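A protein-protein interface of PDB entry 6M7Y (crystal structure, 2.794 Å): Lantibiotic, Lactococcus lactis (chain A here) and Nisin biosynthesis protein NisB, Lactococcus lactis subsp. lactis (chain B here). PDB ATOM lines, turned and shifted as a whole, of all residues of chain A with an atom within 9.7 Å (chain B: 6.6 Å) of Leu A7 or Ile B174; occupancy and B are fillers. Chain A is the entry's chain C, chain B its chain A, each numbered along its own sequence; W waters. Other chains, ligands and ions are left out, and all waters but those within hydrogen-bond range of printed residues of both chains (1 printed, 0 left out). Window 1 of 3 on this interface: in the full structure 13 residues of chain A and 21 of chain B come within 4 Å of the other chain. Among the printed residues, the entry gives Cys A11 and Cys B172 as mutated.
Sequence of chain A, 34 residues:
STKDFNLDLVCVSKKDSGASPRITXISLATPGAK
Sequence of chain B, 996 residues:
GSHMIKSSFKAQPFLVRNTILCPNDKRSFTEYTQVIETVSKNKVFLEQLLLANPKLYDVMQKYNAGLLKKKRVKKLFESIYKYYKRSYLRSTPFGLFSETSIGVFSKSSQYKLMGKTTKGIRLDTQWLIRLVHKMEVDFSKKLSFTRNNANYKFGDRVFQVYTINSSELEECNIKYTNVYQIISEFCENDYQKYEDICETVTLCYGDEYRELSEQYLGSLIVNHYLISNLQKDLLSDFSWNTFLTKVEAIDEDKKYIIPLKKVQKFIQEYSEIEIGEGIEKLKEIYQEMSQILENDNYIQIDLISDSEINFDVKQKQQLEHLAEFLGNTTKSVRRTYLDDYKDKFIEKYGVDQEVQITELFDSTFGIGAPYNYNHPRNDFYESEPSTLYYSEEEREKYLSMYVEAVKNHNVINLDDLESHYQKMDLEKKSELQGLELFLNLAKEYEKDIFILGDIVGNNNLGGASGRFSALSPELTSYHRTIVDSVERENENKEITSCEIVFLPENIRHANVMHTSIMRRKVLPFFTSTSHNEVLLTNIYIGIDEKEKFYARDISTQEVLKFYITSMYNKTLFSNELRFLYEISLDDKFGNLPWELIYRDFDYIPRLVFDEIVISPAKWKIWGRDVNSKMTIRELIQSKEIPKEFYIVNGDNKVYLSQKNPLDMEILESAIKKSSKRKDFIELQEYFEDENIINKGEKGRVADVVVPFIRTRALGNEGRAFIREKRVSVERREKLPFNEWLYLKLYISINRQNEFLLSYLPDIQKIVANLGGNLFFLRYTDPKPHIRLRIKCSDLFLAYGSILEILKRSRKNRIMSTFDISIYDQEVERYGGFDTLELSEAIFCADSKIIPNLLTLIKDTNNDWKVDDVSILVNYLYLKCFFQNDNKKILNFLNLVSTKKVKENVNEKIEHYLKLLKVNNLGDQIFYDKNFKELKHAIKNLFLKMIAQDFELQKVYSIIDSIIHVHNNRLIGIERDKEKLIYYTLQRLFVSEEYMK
The side-chain carboxylate (OD2) of Asp A8 is in salt-bridge range of the guanidinium group (NH1) of Arg B157 (2.8 Å).
The side-chain sulfur of Cys A11 forms a disulfide with the side-chain sulfur of Cys B172, at 2.1 Å.
The backbone NH of Asn B173 sits at hydrogen-bond distance from the backbone carbonyl oxygen of Val A10.
The backbone NH of Lys B175 is in hydrogen-bond range of the backbone carbonyl oxygen of Leu A7 (3.0 Å).
The side-chain hydroxyl (OG1) of Thr B177 lies close to the backbone carbonyl oxygen (O) of Asp A4 (3.3 Å).
The guanidinium group (NE) of Arg B157 sits close to the backbone carbonyl oxygen (O) of Ile B174 (3.3 Å).
The backbone carbonyl oxygen (O) of Ile B174 sits at hydrogen-bond distance from the backbone NH (N) of Val B158.
The side-chain hydroxyl (OG1) of Thr B177 sits at hydrogen-bond distance from the backbone NH (N) of Tyr B180 (2.9 Å).
The side-chain hydroxyl (OG) of Ser B219 lies within hydrogen-bond range of the backbone carbonyl oxygen (O) of Tyr B216 (2.7 Å).
The backbone carbonyl oxygen (O) of Ser B219 sits at hydrogen-bond distance from the side-chain amide nitrogen (ND2) of Asn B223.
O of Leu B220 sits at hydrogen-bond distance from N of Tyr B225 (2.9 Å).
Among the printed residues, pairs that only touch across the chains: Phe A5 with Tyr B216, Leu A7 with Ile B174, Val A10 with Cys B172, Leu A9 with Asn B173, Val A10 with Arg B157, Leu A7 with Tyr B216, Leu A9 with Ile B174, Asn A6 with Tyr B216, Leu A7 with Leu B220, Leu A7 with Ser B219, Leu A9 with Asn B223 and Asp A8 with Asn B173.
Leu A7 touches five residues of chain B.
Of chain A, only Leu A7 (3.3 Å) and Leu A9 (3.7 Å) come within 4 Å of Ile B174.
No residue of chain A comes within 4 Å of Val B158.
Printed residues of chain B within 4 Å of Asp A4: Thr B177.
Printed residues of chain A within 4 Å of Leu B220: Leu A7 (3.9 Å).
Printed residues of chain B within 4 Å of Phe A5: Tyr B216 (3.0 Å).
Printed residues of chain A within 4 Å of Ser B219: Leu A7.
Phe B159 touches none of the printed residues of chain A.
The nearest residue of chain A that does not touch Ile B174 is Asp A8 (4.4 Å).
The nearest printed residue of chain B that does not touch Cys A11 is Asn B173 (5.2 Å).
Printed residues of chain B that touch a printed residue of chain A: Arg B157, Cys B172, Asn B173, Ile B174, Lys B175, Thr B177, Tyr B216, Ser B219, Leu B220 and Asn B223.
Hydrophobic or aromatic side chains of chain B that line the printed part of chain A: Ile B174, Tyr B216 and Leu B220.
Along chain B the printed residues that touch a printed residue of chain A span positions 157 to 223.
Hydrophobic or aromatic side chains of chain A that line the printed part of chain B: Leu A7, Leu A9 and Val A10.
Among the printed residues, 17 pairs touch across the chains.
Among the printed residues, Asp or Glu carboxylates within 4 Å of a Lys or Arg side-chain nitrogen of the other chain: Asp A8 with Arg B157 (2.8 Å).
Water W1 bridges the backbone carbonyl oxygen of Asn A6 (3.3 Å) and the side-chain hydroxyl of Ser B219 (3.5 Å).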
ATOM      1  N   LYS A   3      -0.925 -30.170   9.452  1.00  0.00           N
ATOM      2  CA  LYS A   3      -0.573 -28.749   9.370  1.00  0.00           C
ATOM      3  C   LYS A   3       0.146 -28.290  10.633  1.00  0.00           C
ATOM      4  O   LYS A   3      -0.244 -27.305  11.256  1.00  0.00           O
ATOM      5  CB  LYS A   3      -1.813 -27.896   9.124  1.00  0.00           C
ATOM      6  CG  LYS A   3      -2.626 -28.195   7.860  1.00  0.00           C
ATOM      7  CD  LYS A   3      -1.770 -28.721   6.733  1.00  0.00           C
ATOM      8  CE  LYS A   3      -2.027 -30.191   6.489  1.00  0.00           C
ATOM      9  NZ  LYS A   3      -1.037 -30.712   5.513  1.00  0.00           N
ATOM     10  N   ASP A   4       1.181 -29.015  11.067  1.00  0.00           N
ATOM     11  CA  ASP A   4       2.177 -28.422  11.945  1.00  0.00           C
ATOM     12  C   ASP A   4       3.374 -27.932  11.144  1.00  0.00           C
ATOM     13  O   ASP A   4       4.522 -27.955  11.611  1.00  0.00           O
ATOM     14  CB  ASP A   4       2.585 -29.356  13.097  1.00  0.00           C
ATOM     15  CG  ASP A   4       2.764 -30.792  12.686  1.00  0.00           C
ATOM     16  OD1 ASP A   4       3.370 -31.031  11.628  1.00  0.00           O
ATOM     17  OD2 ASP A   4       2.320 -31.689  13.446  1.00  0.00           O
ATOM     18  N   PHE A   5       3.098 -27.479   9.926  1.00  0.00           N
ATOM     19  CA  PHE A   5       3.983 -26.605   9.178  1.00  0.00           C
ATOM     20  C   PHE A   5       3.556 -25.137   9.266  1.00  0.00           C
ATOM     21  O   PHE A   5       4.028 -24.321   8.456  1.00  0.00           O
ATOM     22  CB  PHE A   5       4.037 -27.040   7.711  1.00  0.00           C
ATOM     23  CG  PHE A   5       4.726 -28.347   7.482  1.00  0.00           C
ATOM     24  CD1 PHE A   5       4.082 -29.543   7.746  1.00  0.00           C
ATOM     25  CD2 PHE A   5       6.021 -28.381   6.971  1.00  0.00           C
ATOM     26  CE1 PHE A   5       4.721 -30.751   7.537  1.00  0.00           C
ATOM     27  CE2 PHE A   5       6.674 -29.585   6.748  1.00  0.00           C
ATOM     28  CZ  PHE A   5       6.023 -30.775   7.029  1.00  0.00           C
ATOM     29  N   ASN A   6       2.674 -24.785  10.230  1.00  0.00           N
ATOM     30  CA  ASN A   6       2.064 -23.448  10.271  1.00  0.00           C
ATOM     31  C   ASN A   6       3.104 -22.342  10.408  1.00  0.00           C
ATOM     32  O   ASN A   6       3.478 -21.729   9.404  1.00  0.00           O
ATOM     33  CB  ASN A   6       1.049 -23.294  11.416  1.00  0.00           C
ATOM     34  CG  ASN A   6       0.211 -21.982  11.321  1.00  0.00           C
ATOM     35  OD1 ASN A   6       0.559 -21.038  10.614  1.00  0.00           O
ATOM     36  ND2 ASN A   6      -0.931 -21.964  12.019  1.00  0.00           N
ATOM     37  N   LEU A   7       3.541 -22.081  11.641  1.00  0.00           N
ATOM     38  CA  LEU A   7       4.473 -21.025  12.061  1.00  0.00           C
ATOM     39  C   LEU A   7       3.736 -20.020  12.916  1.00  0.00           C
ATOM     40  O   LEU A   7       4.249 -19.596  13.956  1.00  0.00           O
ATOM     41  CB  LEU A   7       5.140 -20.266  10.914  1.00  0.00           C
ATOM     42  CG  LEU A   7       6.164 -19.212  11.308  1.00  0.00           C
ATOM     43  CD1 LEU A   7       7.528 -19.857  11.500  1.00  0.00           C
ATOM     44  CD2 LEU A   7       6.259 -18.059  10.293  1.00  0.00           C
ATOM     45  N   ASP A   8       2.566 -19.599  12.449  1.00  0.00           N
ATOM     46  CA  ASP A   8       1.635 -18.832  13.265  1.00  0.00           C
ATOM     47  C   ASP A   8       2.316 -17.617  13.889  1.00  0.00           C
ATOM     48  O   ASP A   8       2.137 -17.320  15.069  1.00  0.00           O
ATOM     49  CB  ASP A   8       1.011 -19.727  14.341  1.00  0.00           C
ATOM     50  CG  ASP A   8      -0.136 -19.052  15.074  1.00  0.00           C
ATOM     51  OD1 ASP A   8      -0.917 -18.331  14.413  1.00  0.00           O
ATOM     52  OD2 ASP A   8      -0.247 -19.243  16.307  1.00  0.00           O
ATOM     53  N   LEU A   9       3.139 -16.924  13.096  1.00  0.00           N
ATOM     54  CA  LEU A   9       3.810 -15.732  13.597  1.00  0.00           C
ATOM     55  C   LEU A   9       2.791 -14.748  14.170  1.00  0.00           C
ATOM     56  O   LEU A   9       1.765 -14.455  13.547  1.00  0.00           O
ATOM     57  CB  LEU A   9       4.627 -15.077  12.484  1.00  0.00           C
ATOM     58  CG  LEU A   9       5.554 -13.908  12.861  1.00  0.00           C
ATOM     59  CD1 LEU A   9       6.913 -14.447  13.226  1.00  0.00           C
ATOM     60  CD2 LEU A   9       5.698 -12.868  11.747  1.00  0.00           C
ATOM     61  N   VAL A  10       3.044 -14.297  15.398  1.00  0.00           N
ATOM     62  CA  VAL A  10       2.254 -13.257  16.048  1.00  0.00           C
ATOM     63  C   VAL A  10       3.224 -12.204  16.568  1.00  0.00           C
ATOM     64  O   VAL A  10       4.343 -12.524  16.988  1.00  0.00           O
ATOM     65  CB  VAL A  10       1.358 -13.817  17.183  1.00  0.00           C
ATOM     66  CG1 VAL A  10       0.764 -15.147  16.777  1.00  0.00           C
ATOM     67  CG2 VAL A  10       2.084 -13.942  18.474  1.00  0.00           C
ATOM     68  N   CYS A  11       2.817 -10.945  16.488  1.00  0.00           N
ATOM     69  CA  CYS A  11       3.670  -9.835  16.864  1.00  0.00           C
ATOM     70  C   CYS A  11       2.884  -8.907  17.773  1.00  0.00           C
ATOM     71  O   CYS A  11       1.671  -8.754  17.616  1.00  0.00           O
ATOM     72  CB  CYS A  11       4.196  -9.084  15.627  1.00  0.00           C
ATOM     73  SG  CYS A  11       5.249 -10.122  14.530  1.00  0.00           S
ATOM     74  N   ASP B 156       3.815 -23.757  24.070  1.00  0.00           N
ATOM     75  CA  ASP B 156       3.567 -23.986  22.657  1.00  0.00           C
ATOM     76  C   ASP B 156       4.121 -22.876  21.768  1.00  0.00           C
ATOM     77  O   ASP B 156       3.739 -22.795  20.594  1.00  0.00           O
ATOM     78  CB  ASP B 156       2.068 -24.134  22.427  1.00  0.00           C
ATOM     79  CG  ASP B 156       1.303 -22.836  22.682  1.00  0.00           C
ATOM     80  OD1 ASP B 156       1.890 -21.894  23.251  1.00  0.00           O
ATOM     81  OD2 ASP B 156       0.101 -22.752  22.319  1.00  0.00           O
ATOM     82  N   ARG B 157       4.992 -22.010  22.290  1.00  0.00           N
ATOM     83  CA  ARG B 157       5.576 -20.940  21.497  1.00  0.00           C
ATOM     84  C   ARG B 157       7.099 -21.046  21.481  1.00  0.00           C
ATOM     85  O   ARG B 157       7.713 -21.563  22.420  1.00  0.00           O
ATOM     86  CB  ARG B 157       5.173 -19.549  22.024  1.00  0.00           C
ATOM     87  CG  ARG B 157       3.690 -19.331  22.214  1.00  0.00           C
ATOM     88  CD  ARG B 157       2.884 -19.516  20.943  1.00  0.00           C
ATOM     89  NE  ARG B 157       3.266 -18.618  19.851  1.00  0.00           N
ATOM     90  CZ  ARG B 157       2.671 -18.592  18.659  1.00  0.00           C
ATOM     91  NH1 ARG B 157       1.657 -19.405  18.397  1.00  0.00           N
ATOM     92  NH2 ARG B 157       3.091 -17.755  17.723  1.00  0.00           N
ATOM     93  N   VAL B 158       7.710 -20.541  20.410  1.00  0.00           N
ATOM     94  CA  VAL B 158       9.151 -20.323  20.344  1.00  0.00           C
ATOM     95  C   VAL B 158       9.404 -18.824  20.392  1.00  0.00           C
ATOM     96  O   VAL B 158       8.952 -18.086  19.509  1.00  0.00           O
ATOM     97  CB  VAL B 158       9.767 -20.912  19.072  1.00  0.00           C
ATOM     98  CG1 VAL B 158      11.247 -20.605  19.040  1.00  0.00           C
ATOM     99  CG2 VAL B 158       9.495 -22.402  18.995  1.00  0.00           C
ATOM    100  N   PHE B 159      10.145 -18.377  21.402  1.00  0.00           N
ATOM    101  CA  PHE B 159      10.448 -16.969  21.592  1.00  0.00           C
ATOM    102  C   PHE B 159      11.908 -16.710  21.267  1.00  0.00           C
ATOM    103  O   PHE B 159      12.695 -17.635  21.092  1.00  0.00           O
ATOM    104  CB  PHE B 159      10.166 -16.537  23.034  1.00  0.00           C
ATOM    105  CG  PHE B 159       8.710 -16.402  23.370  1.00  0.00           C
ATOM    106  CD1 PHE B 159       8.040 -15.218  23.129  1.00  0.00           C
ATOM    107  CD2 PHE B 159       8.018 -17.451  23.969  1.00  0.00           C
ATOM    108  CE1 PHE B 159       6.698 -15.081  23.462  1.00  0.00           C
ATOM    109  CE2 PHE B 159       6.667 -17.318  24.310  1.00  0.00           C
ATOM    110  CZ  PHE B 159       6.015 -16.135  24.063  1.00  0.00           C
ATOM    111  N   CYS B 172       8.267 -10.547  18.044  1.00  0.00           N
ATOM    112  CA  CYS B 172       7.559 -11.559  17.268  1.00  0.00           C
ATOM    113  C   CYS B 172       7.945 -12.958  17.738  1.00  0.00           C
ATOM    114  O   CYS B 172       9.128 -13.227  17.970  1.00  0.00           O
ATOM    115  CB  CYS B 172       7.867 -11.392  15.764  1.00  0.00           C
ATOM    116  SG  CYS B 172       7.248  -9.834  14.996  1.00  0.00           S
ATOM    117  N   ASN B 173       6.954 -13.848  17.859  1.00  0.00           N
ATOM    118  CA  ASN B 173       7.177 -15.234  18.278  1.00  0.00           C
ATOM    119  C   ASN B 173       6.370 -16.176  17.390  1.00  0.00           C
ATOM    120  O   ASN B 173       5.411 -15.766  16.738  1.00  0.00           O
ATOM    121  CB  ASN B 173       6.797 -15.465  19.748  1.00  0.00           C
ATOM    122  CG  ASN B 173       5.308 -15.229  20.013  1.00  0.00           C
ATOM    123  OD1 ASN B 173       4.510 -16.157  20.074  1.00  0.00           O
ATOM    124  ND2 ASN B 173       4.941 -13.978  20.158  1.00  0.00           N
ATOM    125  N   ILE B 174       6.756 -17.457  17.379  1.00  0.00           N
ATOM    126  CA  ILE B 174       6.176 -18.464  16.490  1.00  0.00           C
ATOM    127  C   ILE B 174       5.696 -19.660  17.315  1.00  0.00           C
ATOM    128  O   ILE B 174       6.037 -19.815  18.484  1.00  0.00           O
ATOM    129  CB  ILE B 174       7.179 -18.934  15.409  1.00  0.00           C
ATOM    130  CG1 ILE B 174       8.300 -19.761  16.036  1.00  0.00           C
ATOM    131  CG2 ILE B 174       7.807 -17.761  14.700  1.00  0.00           C
ATOM    132  CD1 ILE B 174       9.374 -20.071  15.074  1.00  0.00           C
ATOM    133  N   LYS B 175       4.904 -20.526  16.686  1.00  0.00           N
ATOM    134  CA  LYS B 175       4.425 -21.731  17.351  1.00  0.00           C
ATOM    135  C   LYS B 175       5.523 -22.789  17.403  1.00  0.00           C
ATOM    136  O   LYS B 175       6.334 -22.914  16.481  1.00  0.00           O
ATOM    137  CB  LYS B 175       3.191 -22.289  16.636  1.00  0.00           C
ATOM    138  CG  LYS B 175       2.525 -23.473  17.343  1.00  0.00           C
ATOM    139  CD  LYS B 175       0.978 -23.396  17.266  1.00  0.00           C
ATOM    140  CE  LYS B 175       0.269 -24.683  17.781  1.00  0.00           C
ATOM    141  NZ  LYS B 175       0.397 -25.036  19.271  1.00  0.00           N
ATOM    142  N   TYR B 176       5.562 -23.533  18.504  1.00  0.00           N
ATOM    143  CA  TYR B 176       6.407 -24.715  18.606  1.00  0.00           C
ATOM    144  C   TYR B 176       5.678 -25.855  17.916  1.00  0.00           C
ATOM    145  O   TYR B 176       4.818 -26.506  18.513  1.00  0.00           O
ATOM    146  CB  TYR B 176       6.705 -25.066  20.062  1.00  0.00           C
ATOM    147  CG  TYR B 176       7.787 -26.125  20.226  1.00  0.00           C
ATOM    148  CD1 TYR B 176       9.139 -25.767  20.226  1.00  0.00           C
ATOM    149  CD2 TYR B 176       7.463 -27.478  20.348  1.00  0.00           C
ATOM    150  CE1 TYR B 176      10.146 -26.719  20.360  1.00  0.00           C
ATOM    151  CE2 TYR B 176       8.463 -28.450  20.482  1.00  0.00           C
ATOM    152  CZ  TYR B 176       9.807 -28.066  20.497  1.00  0.00           C
ATOM    153  OH  TYR B 176      10.825 -29.012  20.639  1.00  0.00           O
ATOM    154  N   THR B 177       6.024 -26.106  16.658  1.00  0.00           N
ATOM    155  CA  THR B 177       5.452 -27.188  15.866  1.00  0.00           C
ATOM    156  C   THR B 177       6.373 -28.400  15.845  1.00  0.00           C
ATOM    157  O   THR B 177       7.584 -28.304  16.079  1.00  0.00           O
ATOM    158  CB  THR B 177       5.195 -26.731  14.426  1.00  0.00           C
ATOM    159  OG1 THR B 177       6.438 -26.354  13.811  1.00  0.00           O
ATOM    160  CG2 THR B 177       4.224 -25.560  14.391  1.00  0.00           C
ATOM    161  N   TYR B 180       9.161 -27.345  13.633  1.00  0.00           N
ATOM    162  CA  TYR B 180      10.204 -26.557  14.282  1.00  0.00           C
ATOM    163  C   TYR B 180      11.134 -27.458  15.084  1.00  0.00           C
ATOM    164  O   TYR B 180      12.360 -27.284  15.061  1.00  0.00           O
ATOM    165  CB  TYR B 180       9.623 -25.472  15.193  1.00  0.00           C
ATOM    166  CG  TYR B 180      10.739 -24.737  15.915  1.00  0.00           C
ATOM    167  CD1 TYR B 180      11.460 -23.729  15.276  1.00  0.00           C
ATOM    168  CD2 TYR B 180      11.113 -25.083  17.217  1.00  0.00           C
ATOM    169  CE1 TYR B 180      12.511 -23.064  15.922  1.00  0.00           C
ATOM    170  CE2 TYR B 180      12.171 -24.434  17.868  1.00  0.00           C
ATOM    171  CZ  TYR B 180      12.867 -23.423  17.221  1.00  0.00           C
ATOM    172  OH  TYR B 180      13.921 -22.779  17.868  1.00  0.00           O
ATOM    173  N   TYR B 216       8.390 -23.596   5.078  1.00  0.00           N
ATOM    174  CA  TYR B 216       8.600 -23.452   6.510  1.00  0.00           C
ATOM    175  C   TYR B 216      10.053 -23.157   6.801  1.00  0.00           C
ATOM    176  O   TYR B 216      10.365 -22.345   7.677  1.00  0.00           O
ATOM    177  CB  TYR B 216       8.158 -24.702   7.271  1.00  0.00           C
ATOM    178  CG  TYR B 216       8.033 -24.478   8.774  1.00  0.00           C
ATOM    179  CD1 TYR B 216       6.859 -23.981   9.317  1.00  0.00           C
ATOM    180  CD2 TYR B 216       9.103 -24.743   9.647  1.00  0.00           C
ATOM    181  CE1 TYR B 216       6.730 -23.769  10.691  1.00  0.00           C
ATOM    182  CE2 TYR B 216       8.988 -24.521  11.034  1.00  0.00           C
ATOM    183  CZ  TYR B 216       7.790 -24.037  11.550  1.00  0.00           C
ATOM    184  OH  TYR B 216       7.620 -23.814  12.911  1.00  0.00           O
ATOM    185  N   SER B 219      10.876 -19.528   5.939  1.00  0.00           N
ATOM    186  CA  SER B 219      10.294 -18.575   6.868  1.00  0.00           C
ATOM    187  C   SER B 219      11.096 -18.494   8.160  1.00  0.00           C
ATOM    188  O   SER B 219      11.196 -17.411   8.754  1.00  0.00           O
ATOM    189  CB  SER B 219       8.839 -18.947   7.137  1.00  0.00           C
ATOM    190  OG  SER B 219       8.753 -20.208   7.772  1.00  0.00           O
ATOM    191  N   LEU B 220      11.690 -19.613   8.599  1.00  0.00           N
ATOM    192  CA  LEU B 220      12.639 -19.549   9.705  1.00  0.00           C
ATOM    193  C   LEU B 220      13.853 -18.695   9.359  1.00  0.00           C
ATOM    194  O   LEU B 220      14.450 -18.081  10.251  1.00  0.00           O
ATOM    195  CB  LEU B 220      13.096 -20.947  10.105  1.00  0.00           C
ATOM    196  CG  LEU B 220      12.106 -22.059  10.407  1.00  0.00           C
ATOM    197  CD1 LEU B 220      12.863 -23.251  10.976  1.00  0.00           C
ATOM    198  CD2 LEU B 220      11.034 -21.608  11.395  1.00  0.00           C
ATOM    199  N   ASN B 223      12.901 -14.723   9.325  1.00  0.00           N
ATOM    200  CA  ASN B 223      12.751 -14.297  10.714  1.00  0.00           C
ATOM    201  C   ASN B 223      13.982 -14.583  11.584  1.00  0.00           C
ATOM    202  O   ASN B 223      13.972 -14.244  12.763  1.00  0.00           O
ATOM    203  CB  ASN B 223      11.498 -14.953  11.292  1.00  0.00           C
ATOM    204  CG  ASN B 223      10.259 -14.604  10.490  1.00  0.00           C
ATOM    205  OD1 ASN B 223       9.748 -13.499  10.587  1.00  0.00           O
ATOM    206  ND2 ASN B 223       9.803 -15.530   9.653  1.00  0.00           N
ATOM    207  N   TYR B 225      15.210 -17.181  12.874  1.00  0.00           N
ATOM    208  CA  TYR B 225      15.307 -18.307  13.777  1.00  0.00           C
ATOM    209  C   TYR B 225      16.466 -19.231  13.420  1.00  0.00           C
ATOM    210  O   TYR B 225      16.839 -20.061  14.258  1.00  0.00           O
ATOM    211  CB  TYR B 225      13.989 -19.058  13.798  1.00  0.00           C
ATOM    212  CG  TYR B 225      12.955 -18.316  14.590  1.00  0.00           C
ATOM    213  CD1 TYR B 225      12.258 -17.238  14.036  1.00  0.00           C
ATOM    214  CD2 TYR B 225      12.682 -18.661  15.911  1.00  0.00           C
ATOM    215  CE1 TYR B 225      11.299 -16.533  14.778  1.00  0.00           C
ATOM    216  CE2 TYR B 225      11.718 -17.968  16.653  1.00  0.00           C
ATOM    217  CZ  TYR B 225      11.033 -16.912  16.080  1.00  0.00           C
ATOM    218  OH  TYR B 225      10.087 -16.242  16.821  1.00  0.00           O
HETATM  219  O   HOH W   1       5.317 -20.228   7.157  1.00  0.00           O
